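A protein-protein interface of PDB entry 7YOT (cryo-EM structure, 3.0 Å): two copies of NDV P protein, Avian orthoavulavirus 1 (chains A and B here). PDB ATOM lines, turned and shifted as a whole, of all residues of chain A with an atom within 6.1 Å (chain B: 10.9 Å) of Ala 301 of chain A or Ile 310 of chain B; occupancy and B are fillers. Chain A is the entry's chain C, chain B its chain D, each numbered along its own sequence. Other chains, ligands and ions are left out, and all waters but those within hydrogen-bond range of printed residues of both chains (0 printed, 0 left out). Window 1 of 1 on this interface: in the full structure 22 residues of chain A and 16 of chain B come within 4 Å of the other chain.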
ATOM      1  N   ASN A 292       3.926   2.632 -17.732  1.00  0.00           N
ATOM      2  CA  ASN A 292       4.565   3.055 -18.968  1.00  0.00           C
ATOM      3  C   ASN A 292       3.617   3.043 -20.156  1.00  0.00           C
ATOM      4  O   ASN A 292       4.056   3.265 -21.284  1.00  0.00           O
ATOM      5  CB  ASN A 292       5.802   2.206 -19.284  1.00  0.00           C
ATOM      6  CG  ASN A 292       5.498   0.728 -19.502  1.00  0.00           C
ATOM      7  OD1 ASN A 292       4.364   0.262 -19.384  1.00  0.00           O
ATOM      8  ND2 ASN A 292       6.543  -0.024 -19.820  1.00  0.00           N
ATOM      9  N   VAL A 293       2.344   2.744 -19.937  1.00  0.00           N
ATOM     10  CA  VAL A 293       1.349   2.862 -20.993  1.00  0.00           C
ATOM     11  C   VAL A 293       1.057   4.347 -21.142  1.00  0.00           C
ATOM     12  O   VAL A 293       0.536   4.972 -20.218  1.00  0.00           O
ATOM     13  CB  VAL A 293       0.076   2.078 -20.665  1.00  0.00           C
ATOM     14  CG1 VAL A 293      -0.922   2.213 -21.786  1.00  0.00           C
ATOM     15  CG2 VAL A 293       0.393   0.631 -20.398  1.00  0.00           C
ATOM     16  N   SER A 294       1.427   4.923 -22.283  1.00  0.00           N
ATOM     17  CA  SER A 294       1.196   6.342 -22.494  1.00  0.00           C
ATOM     18  C   SER A 294      -0.291   6.616 -22.633  1.00  0.00           C
ATOM     19  O   SER A 294      -1.054   5.777 -23.107  1.00  0.00           O
ATOM     20  CB  SER A 294       1.931   6.840 -23.733  1.00  0.00           C
ATOM     21  OG  SER A 294       1.396   6.269 -24.906  1.00  0.00           O
ATOM     22  N   SER A 297      -3.054   6.706 -26.191  1.00  0.00           N
ATOM     23  CA  SER A 297      -3.165   5.387 -26.782  1.00  0.00           C
ATOM     24  C   SER A 297      -4.589   4.887 -26.611  1.00  0.00           C
ATOM     25  O   SER A 297      -5.261   5.210 -25.629  1.00  0.00           O
ATOM     26  CB  SER A 297      -2.183   4.403 -26.148  1.00  0.00           C
ATOM     27  OG  SER A 297      -2.528   4.147 -24.805  1.00  0.00           O
ATOM     28  N   ASP A 298      -5.043   4.100 -27.579  1.00  0.00           N
ATOM     29  CA  ASP A 298      -6.413   3.617 -27.578  1.00  0.00           C
ATOM     30  C   ASP A 298      -6.577   2.527 -26.536  1.00  0.00           C
ATOM     31  O   ASP A 298      -5.740   1.629 -26.429  1.00  0.00           O
ATOM     32  CB  ASP A 298      -6.792   3.078 -28.953  1.00  0.00           C
ATOM     33  CG  ASP A 298      -6.801   4.150 -30.009  1.00  0.00           C
ATOM     34  OD1 ASP A 298      -7.027   5.325 -29.658  1.00  0.00           O
ATOM     35  OD2 ASP A 298      -6.584   3.822 -31.190  1.00  0.00           O
ATOM     36  N   LEU A 299      -7.661   2.604 -25.767  1.00  0.00           N
ATOM     37  CA  LEU A 299      -7.866   1.644 -24.694  1.00  0.00           C
ATOM     38  C   LEU A 299      -8.295   0.274 -25.200  1.00  0.00           C
ATOM     39  O   LEU A 299      -8.069  -0.721 -24.503  1.00  0.00           O
ATOM     40  CB  LEU A 299      -8.882   2.184 -23.687  1.00  0.00           C
ATOM     41  CG  LEU A 299      -8.407   3.366 -22.846  1.00  0.00           C
ATOM     42  CD1 LEU A 299      -9.518   3.894 -21.988  1.00  0.00           C
ATOM     43  CD2 LEU A 299      -7.249   2.970 -21.977  1.00  0.00           C
ATOM     44  N   ARG A 300      -8.887   0.192 -26.392  1.00  0.00           N
ATOM     45  CA  ARG A 300      -9.070  -1.110 -27.021  1.00  0.00           C
ATOM     46  C   ARG A 300      -7.732  -1.732 -27.378  1.00  0.00           C
ATOM     47  O   ARG A 300      -7.566  -2.951 -27.302  1.00  0.00           O
ATOM     48  CB  ARG A 300      -9.901  -1.004 -28.290  1.00  0.00           C
ATOM     49  CG  ARG A 300     -11.339  -0.591 -28.167  1.00  0.00           C
ATOM     50  CD  ARG A 300     -11.907  -0.733 -29.561  1.00  0.00           C
ATOM     51  NE  ARG A 300     -13.197  -0.101 -29.773  1.00  0.00           N
ATOM     52  CZ  ARG A 300     -13.772  -0.033 -30.966  1.00  0.00           C
ATOM     53  NH1 ARG A 300     -13.168  -0.569 -32.016  1.00  0.00           N
ATOM     54  NH2 ARG A 300     -14.940   0.571 -31.119  1.00  0.00           N
ATOM     55  N   ALA A 301      -6.771  -0.909 -27.796  1.00  0.00           N
ATOM     56  CA  ALA A 301      -5.451  -1.428 -28.119  1.00  0.00           C
ATOM     57  C   ALA A 301      -4.678  -1.818 -26.870  1.00  0.00           C
ATOM     58  O   ALA A 301      -3.838  -2.719 -26.924  1.00  0.00           O
ATOM     59  CB  ALA A 301      -4.671  -0.398 -28.921  1.00  0.00           C
ATOM     60  N   VAL A 302      -4.939  -1.153 -25.746  1.00  0.00           N
ATOM     61  CA  VAL A 302      -4.367  -1.582 -24.476  1.00  0.00           C
ATOM     62  C   VAL A 302      -4.996  -2.897 -24.038  1.00  0.00           C
ATOM     63  O   VAL A 302      -4.315  -3.777 -23.496  1.00  0.00           O
ATOM     64  CB  VAL A 302      -4.545  -0.474 -23.420  1.00  0.00           C
ATOM     65  CG1 VAL A 302      -4.021  -0.904 -22.063  1.00  0.00           C
ATOM     66  CG2 VAL A 302      -3.851   0.785 -23.867  1.00  0.00           C
ATOM     67  N   ALA A 303      -6.294  -3.070 -24.299  1.00  0.00           N
ATOM     68  CA  ALA A 303      -6.970  -4.307 -23.914  1.00  0.00           C
ATOM     69  C   ALA A 303      -6.524  -5.488 -24.766  1.00  0.00           C
ATOM     70  O   ALA A 303      -6.300  -6.583 -24.242  1.00  0.00           O
ATOM     71  CB  ALA A 303      -8.479  -4.129 -24.014  1.00  0.00           C
ATOM     72  N   LYS A 304      -6.379  -5.292 -26.074  1.00  0.00           N
ATOM     73  CA  LYS A 304      -6.041  -6.392 -26.967  1.00  0.00           C
ATOM     74  C   LYS A 304      -4.585  -6.824 -26.880  1.00  0.00           C
ATOM     75  O   LYS A 304      -4.253  -7.904 -27.378  1.00  0.00           O
ATOM     76  CB  LYS A 304      -6.367  -6.021 -28.414  1.00  0.00           C
ATOM     77  CG  LYS A 304      -7.849  -5.930 -28.703  1.00  0.00           C
ATOM     78  CD  LYS A 304      -8.106  -5.570 -30.146  1.00  0.00           C
ATOM     79  CE  LYS A 304      -9.589  -5.426 -30.420  1.00  0.00           C
ATOM     80  NZ  LYS A 304      -9.854  -5.036 -31.833  1.00  0.00           N
ATOM     81  N   SER A 305      -3.714  -6.026 -26.275  1.00  0.00           N
ATOM     82  CA  SER A 305      -2.311  -6.402 -26.165  1.00  0.00           C
ATOM     83  C   SER A 305      -2.117  -7.428 -25.058  1.00  0.00           C
ATOM     84  O   SER A 305      -1.264  -7.260 -24.189  1.00  0.00           O
ATOM     85  CB  SER A 305      -1.438  -5.181 -25.897  1.00  0.00           C
ATOM     86  OG  SER A 305      -1.686  -4.660 -24.606  1.00  0.00           O
ATOM     87  N   VAL B 275     -10.844 -12.966 -27.904  1.00  0.00           N
ATOM     88  CA  VAL B 275      -9.731 -12.175 -27.381  1.00  0.00           C
ATOM     89  C   VAL B 275     -10.008 -11.746 -25.939  1.00  0.00           C
ATOM     90  O   VAL B 275      -9.105 -11.754 -25.088  1.00  0.00           O
ATOM     91  CB  VAL B 275      -9.455 -10.972 -28.307  1.00  0.00           C
ATOM     92  CG1 VAL B 275      -8.404 -10.044 -27.721  1.00  0.00           C
ATOM     93  CG2 VAL B 275      -8.985 -11.455 -29.661  1.00  0.00           C
ATOM     94  N   ASN B 279      -7.872 -12.316 -22.468  1.00  0.00           N
ATOM     95  CA  ASN B 279      -7.386 -11.209 -21.650  1.00  0.00           C
ATOM     96  C   ASN B 279      -7.857 -11.320 -20.207  1.00  0.00           C
ATOM     97  O   ASN B 279      -7.099 -11.003 -19.286  1.00  0.00           O
ATOM     98  CB  ASN B 279      -7.808  -9.876 -22.256  1.00  0.00           C
ATOM     99  CG  ASN B 279      -7.027  -9.544 -23.500  1.00  0.00           C
ATOM    100  OD1 ASN B 279      -5.815  -9.747 -23.556  1.00  0.00           O
ATOM    101  ND2 ASN B 279      -7.713  -9.030 -24.510  1.00  0.00           N
ATOM    102  N   MET B 283      -5.635 -11.556 -16.165  1.00  0.00           N
ATOM    103  CA  MET B 283      -5.732 -10.539 -15.133  1.00  0.00           C
ATOM    104  C   MET B 283      -5.682 -11.171 -13.750  1.00  0.00           C
ATOM    105  O   MET B 283      -5.993 -12.349 -13.564  1.00  0.00           O
ATOM    106  CB  MET B 283      -7.007  -9.722 -15.298  1.00  0.00           C
ATOM    107  CG  MET B 283      -6.989  -8.842 -16.523  1.00  0.00           C
ATOM    108  SD  MET B 283      -8.472  -7.853 -16.710  1.00  0.00           S
ATOM    109  CE  MET B 283      -8.110  -7.059 -18.267  1.00  0.00           C
ATOM    110  N   VAL B 302       9.100  -1.396 -14.677  1.00  0.00           N
ATOM    111  CA  VAL B 302       8.381  -0.733 -15.756  1.00  0.00           C
ATOM    112  C   VAL B 302       8.857   0.703 -15.957  1.00  0.00           C
ATOM    113  O   VAL B 302       8.989   1.169 -17.094  1.00  0.00           O
ATOM    114  CB  VAL B 302       6.878  -0.850 -15.451  1.00  0.00           C
ATOM    115  CG1 VAL B 302       6.069   0.149 -16.184  1.00  0.00           C
ATOM    116  CG2 VAL B 302       6.429  -2.226 -15.901  1.00  0.00           C
ATOM    117  N   SER B 305      12.064   2.573 -18.472  1.00  0.00           N
ATOM    118  CA  SER B 305      12.063   2.861 -19.895  1.00  0.00           C
ATOM    119  C   SER B 305      11.123   4.020 -20.201  1.00  0.00           C
ATOM    120  O   SER B 305      10.347   4.471 -19.356  1.00  0.00           O
ATOM    121  CB  SER B 305      11.669   1.623 -20.713  1.00  0.00           C
ATOM    122  OG  SER B 305      10.331   1.239 -20.457  1.00  0.00           O
ATOM    123  N   HIS B 306      11.230   4.503 -21.434  1.00  0.00           N
ATOM    124  CA  HIS B 306      10.363   5.559 -21.933  1.00  0.00           C
ATOM    125  C   HIS B 306       8.933   5.033 -22.044  1.00  0.00           C
ATOM    126  O   HIS B 306       8.735   3.858 -22.370  1.00  0.00           O
ATOM    127  CB  HIS B 306      10.884   6.020 -23.297  1.00  0.00           C
ATOM    128  CG  HIS B 306      10.150   7.184 -23.884  1.00  0.00           C
ATOM    129  ND1 HIS B 306      10.299   8.472 -23.414  1.00  0.00           N
ATOM    130  CD2 HIS B 306       9.281   7.261 -24.921  1.00  0.00           C
ATOM    131  CE1 HIS B 306       9.543   9.289 -24.126  1.00  0.00           C
ATOM    132  NE2 HIS B 306       8.914   8.579 -25.046  1.00  0.00           N
ATOM    133  N   PRO B 307       7.922   5.851 -21.736  1.00  0.00           N
ATOM    134  CA  PRO B 307       6.532   5.375 -21.826  1.00  0.00           C
ATOM    135  C   PRO B 307       6.115   5.094 -23.263  1.00  0.00           C
ATOM    136  O   PRO B 307       6.300   5.922 -24.157  1.00  0.00           O
ATOM    137  CB  PRO B 307       5.722   6.516 -21.200  1.00  0.00           C
ATOM    138  CG  PRO B 307       6.572   7.697 -21.325  1.00  0.00           C
ATOM    139  CD  PRO B 307       7.987   7.212 -21.182  1.00  0.00           C
ATOM    140  N   VAL B 308       5.551   3.908 -23.474  1.00  0.00           N
ATOM    141  CA  VAL B 308       5.380   3.343 -24.800  1.00  0.00           C
ATOM    142  C   VAL B 308       3.972   3.604 -25.313  1.00  0.00           C
ATOM    143  O   VAL B 308       3.029   3.838 -24.556  1.00  0.00           O
ATOM    144  CB  VAL B 308       5.689   1.831 -24.810  1.00  0.00           C
ATOM    145  CG1 VAL B 308       7.133   1.592 -24.430  1.00  0.00           C
ATOM    146  CG2 VAL B 308       4.767   1.095 -23.861  1.00  0.00           C
ATOM    147  N   LEU B 309       3.833   3.550 -26.632  1.00  0.00           N
ATOM    148  CA  LEU B 309       2.559   3.737 -27.315  1.00  0.00           C
ATOM    149  C   LEU B 309       2.049   2.378 -27.771  1.00  0.00           C
ATOM    150  O   LEU B 309       2.731   1.680 -28.528  1.00  0.00           O
ATOM    151  CB  LEU B 309       2.724   4.674 -28.508  1.00  0.00           C
ATOM    152  CG  LEU B 309       1.460   5.011 -29.285  1.00  0.00           C
ATOM    153  CD1 LEU B 309       0.535   5.722 -28.359  1.00  0.00           C
ATOM    154  CD2 LEU B 309       1.768   5.870 -30.492  1.00  0.00           C
ATOM    155  N   ILE B 310       0.854   2.004 -27.309  1.00  0.00           N
ATOM    156  CA  ILE B 310       0.275   0.702 -27.613  1.00  0.00           C
ATOM    157  C   ILE B 310      -0.849   0.817 -28.644  1.00  0.00           C
ATOM    158  O   ILE B 310      -1.348  -0.204 -29.140  1.00  0.00           O
ATOM    159  CB  ILE B 310      -0.177   0.036 -26.291  1.00  0.00           C
ATOM    160  CG1 ILE B 310       1.002   0.027 -25.331  1.00  0.00           C
ATOM    161  CG2 ILE B 310      -0.482  -1.457 -26.420  1.00  0.00           C
ATOM    162  CD1 ILE B 310       0.657  -0.397 -23.947  1.00  0.00           C
ATOM    163  N   ALA B 311      -1.188   2.040 -29.056  1.00  0.00           N
ATOM    164  CA  ALA B 311      -2.349   2.325 -29.891  1.00  0.00           C
ATOM    165  C   ALA B 311      -2.263   1.668 -31.267  1.00  0.00           C
ATOM    166  O   ALA B 311      -1.199   1.248 -31.732  1.00  0.00           O
ATOM    167  CB  ALA B 311      -2.525   3.829 -30.078  1.00  0.00           C
ATOM    168  N   GLY B 312      -3.422   1.570 -31.906  1.00  0.00           N
ATOM    169  CA  GLY B 312      -3.555   0.967 -33.215  1.00  0.00           C
ATOM    170  C   GLY B 312      -5.021   0.861 -33.578  1.00  0.00           C
ATOM    171  O   GLY B 312      -5.890   1.153 -32.753  1.00  0.00           O
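The side-chain hydroxyl of Ser 297 of chain A is in hydrogen-bond range of the backbone carbonyl oxygen of Ser 294 of chain A (2.8 Å).
The backbone carbonyl oxygen (O) of Val 275 of chain B sits at hydrogen-bond distance from the side-chain amide nitrogen (ND2) of Asn 279 of chain B.
O of Val 302 of chain A sits at hydrogen-bond distance from OG of Ser 305 of chain A (3.0 Å).
The side-chain amide nitrogen (ND2) of Asn 279 of chain B lies within hydrogen-bond range of the backbone carbonyl oxygen (O) of Ala 303 of chain A (2.8 Å).
OD2 of Asp 298 of chain A sits close to O of Gly 312 of chain B, at 3.2 Å.
The backbone NH of Val 308 of chain B is in hydrogen-bond range of the backbone carbonyl oxygen of Asn 292 of chain A, at 2.7 Å.
The side-chain hydroxyl (OG) of Ser 294 of chain A is in hydrogen-bond range of the backbone carbonyl oxygen (O) of Val 308 of chain B.
Positions printed for both chains: 302 and 305.
Of the 17 pairs that touch across the chains among the printed residues, none has its exchanged pair printed and touching as well.
Ala 301 of chain A touches three residues of chain B.
Of chain B, only Val 308 and Ile 310 come within 4 Å of Val 293 of chain A.
Ser 294 of chain A touches just these residues of chain B: Val 308 (2.9 Å) and Leu 309 (3.6 Å).
Of chain B, only Leu 309 (3.7 Å) and Ala 311 (3.7 Å) come within 4 Å of Ser 297 of chain A.
Asp 298 of chain A touches just these residues of chain B: Ala 311 and Gly 312.
No residue of chain B comes within 4 Å of Val 302 of chain A.
Of chain B, only Asn 279 comes within 4 Å of Ala 303 of chain A.
Lys 304 of chain A touches just one residue of chain B: Asn 279.
Ser 305 of chain A touches just one residue of chain B: Ile 310.
Of the printed residues of chain A, Leu 309 of chain B touches Ser 294 and Ser 297.
Printed residues of chain A within 4 Å of Pro 307 of chain B: Asn 292.
Printed residues of chain A within 4 Å of Asn 279 of chain B: Ala 303 and Lys 304.
Printed residues of chain A within 4 Å of Val 308 of chain B: Asn 292, Val 293 and Ser 294.
Of the printed residues of chain A, Ala 311 of chain B touches Ser 297, Asp 298 and Ala 301.
The nearest printed residue of chain A that does not touch Gly 312 of chain B is Ser 297 of chain A (6.4 Å).
O of Val 308 of chain B touches C of Val 293 of chain A (3.98 Å).
Val 293 of chain A touches Ile 310 of chain B.
Ser 294 of chain A touches Leu 309 of chain B (OG to CD1, 3.6 Å).
Leu 309 of chain B touches Ser 297 of chain A.
N of Asp 298 of chain A touches CB of Ala 311 of chain B, 3.6 Å away.
CB of Ala 301 of chain A touches O of Ile 310 of chain B, 3.3 Å away.
Ala 311 of chain B touches Ala 301 of chain A.
Gly 312 of chain B touches Ala 301 of chain A.
Lys 304 of chain A touches Asn 279 of chain B (CA to ND2, 3.97 Å).
Ile 310 of chain B touches Ser 305 of chain A (CG2 to OG, 3.9 Å).
Printed residues of chain A that touch a printed residue of chain B: Asn 292, Val 293, Ser 294, Ser 297, Asp 298, Ala 301, Ala 303, Lys 304 and Ser 305.
Hydrophobic or aromatic side chains of chain A that line the printed part of chain B: Val 293 and Ala 301.
Of the 12 printed residues of chain B, 8 touch a printed residue of chain A.
Printed residues of chain B that touch a printed residue of chain A: Asn 279, Val 302, Pro 307, Val 308, Leu 309, Ile 310, Ala 311 and Gly 312.
Hydrophobic or aromatic side chains of chain B that line the printed part of chain A: Val 302, Pro 307, Val 308, Leu 309, Ile 310 and Ala 311.
Among the printed residues, 17 pairs touch across the chains.
Among the printed residues, no Asp or Glu carboxylate lies within 4 Å of a Lys or Arg side-chain nitrogen of the other chain.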
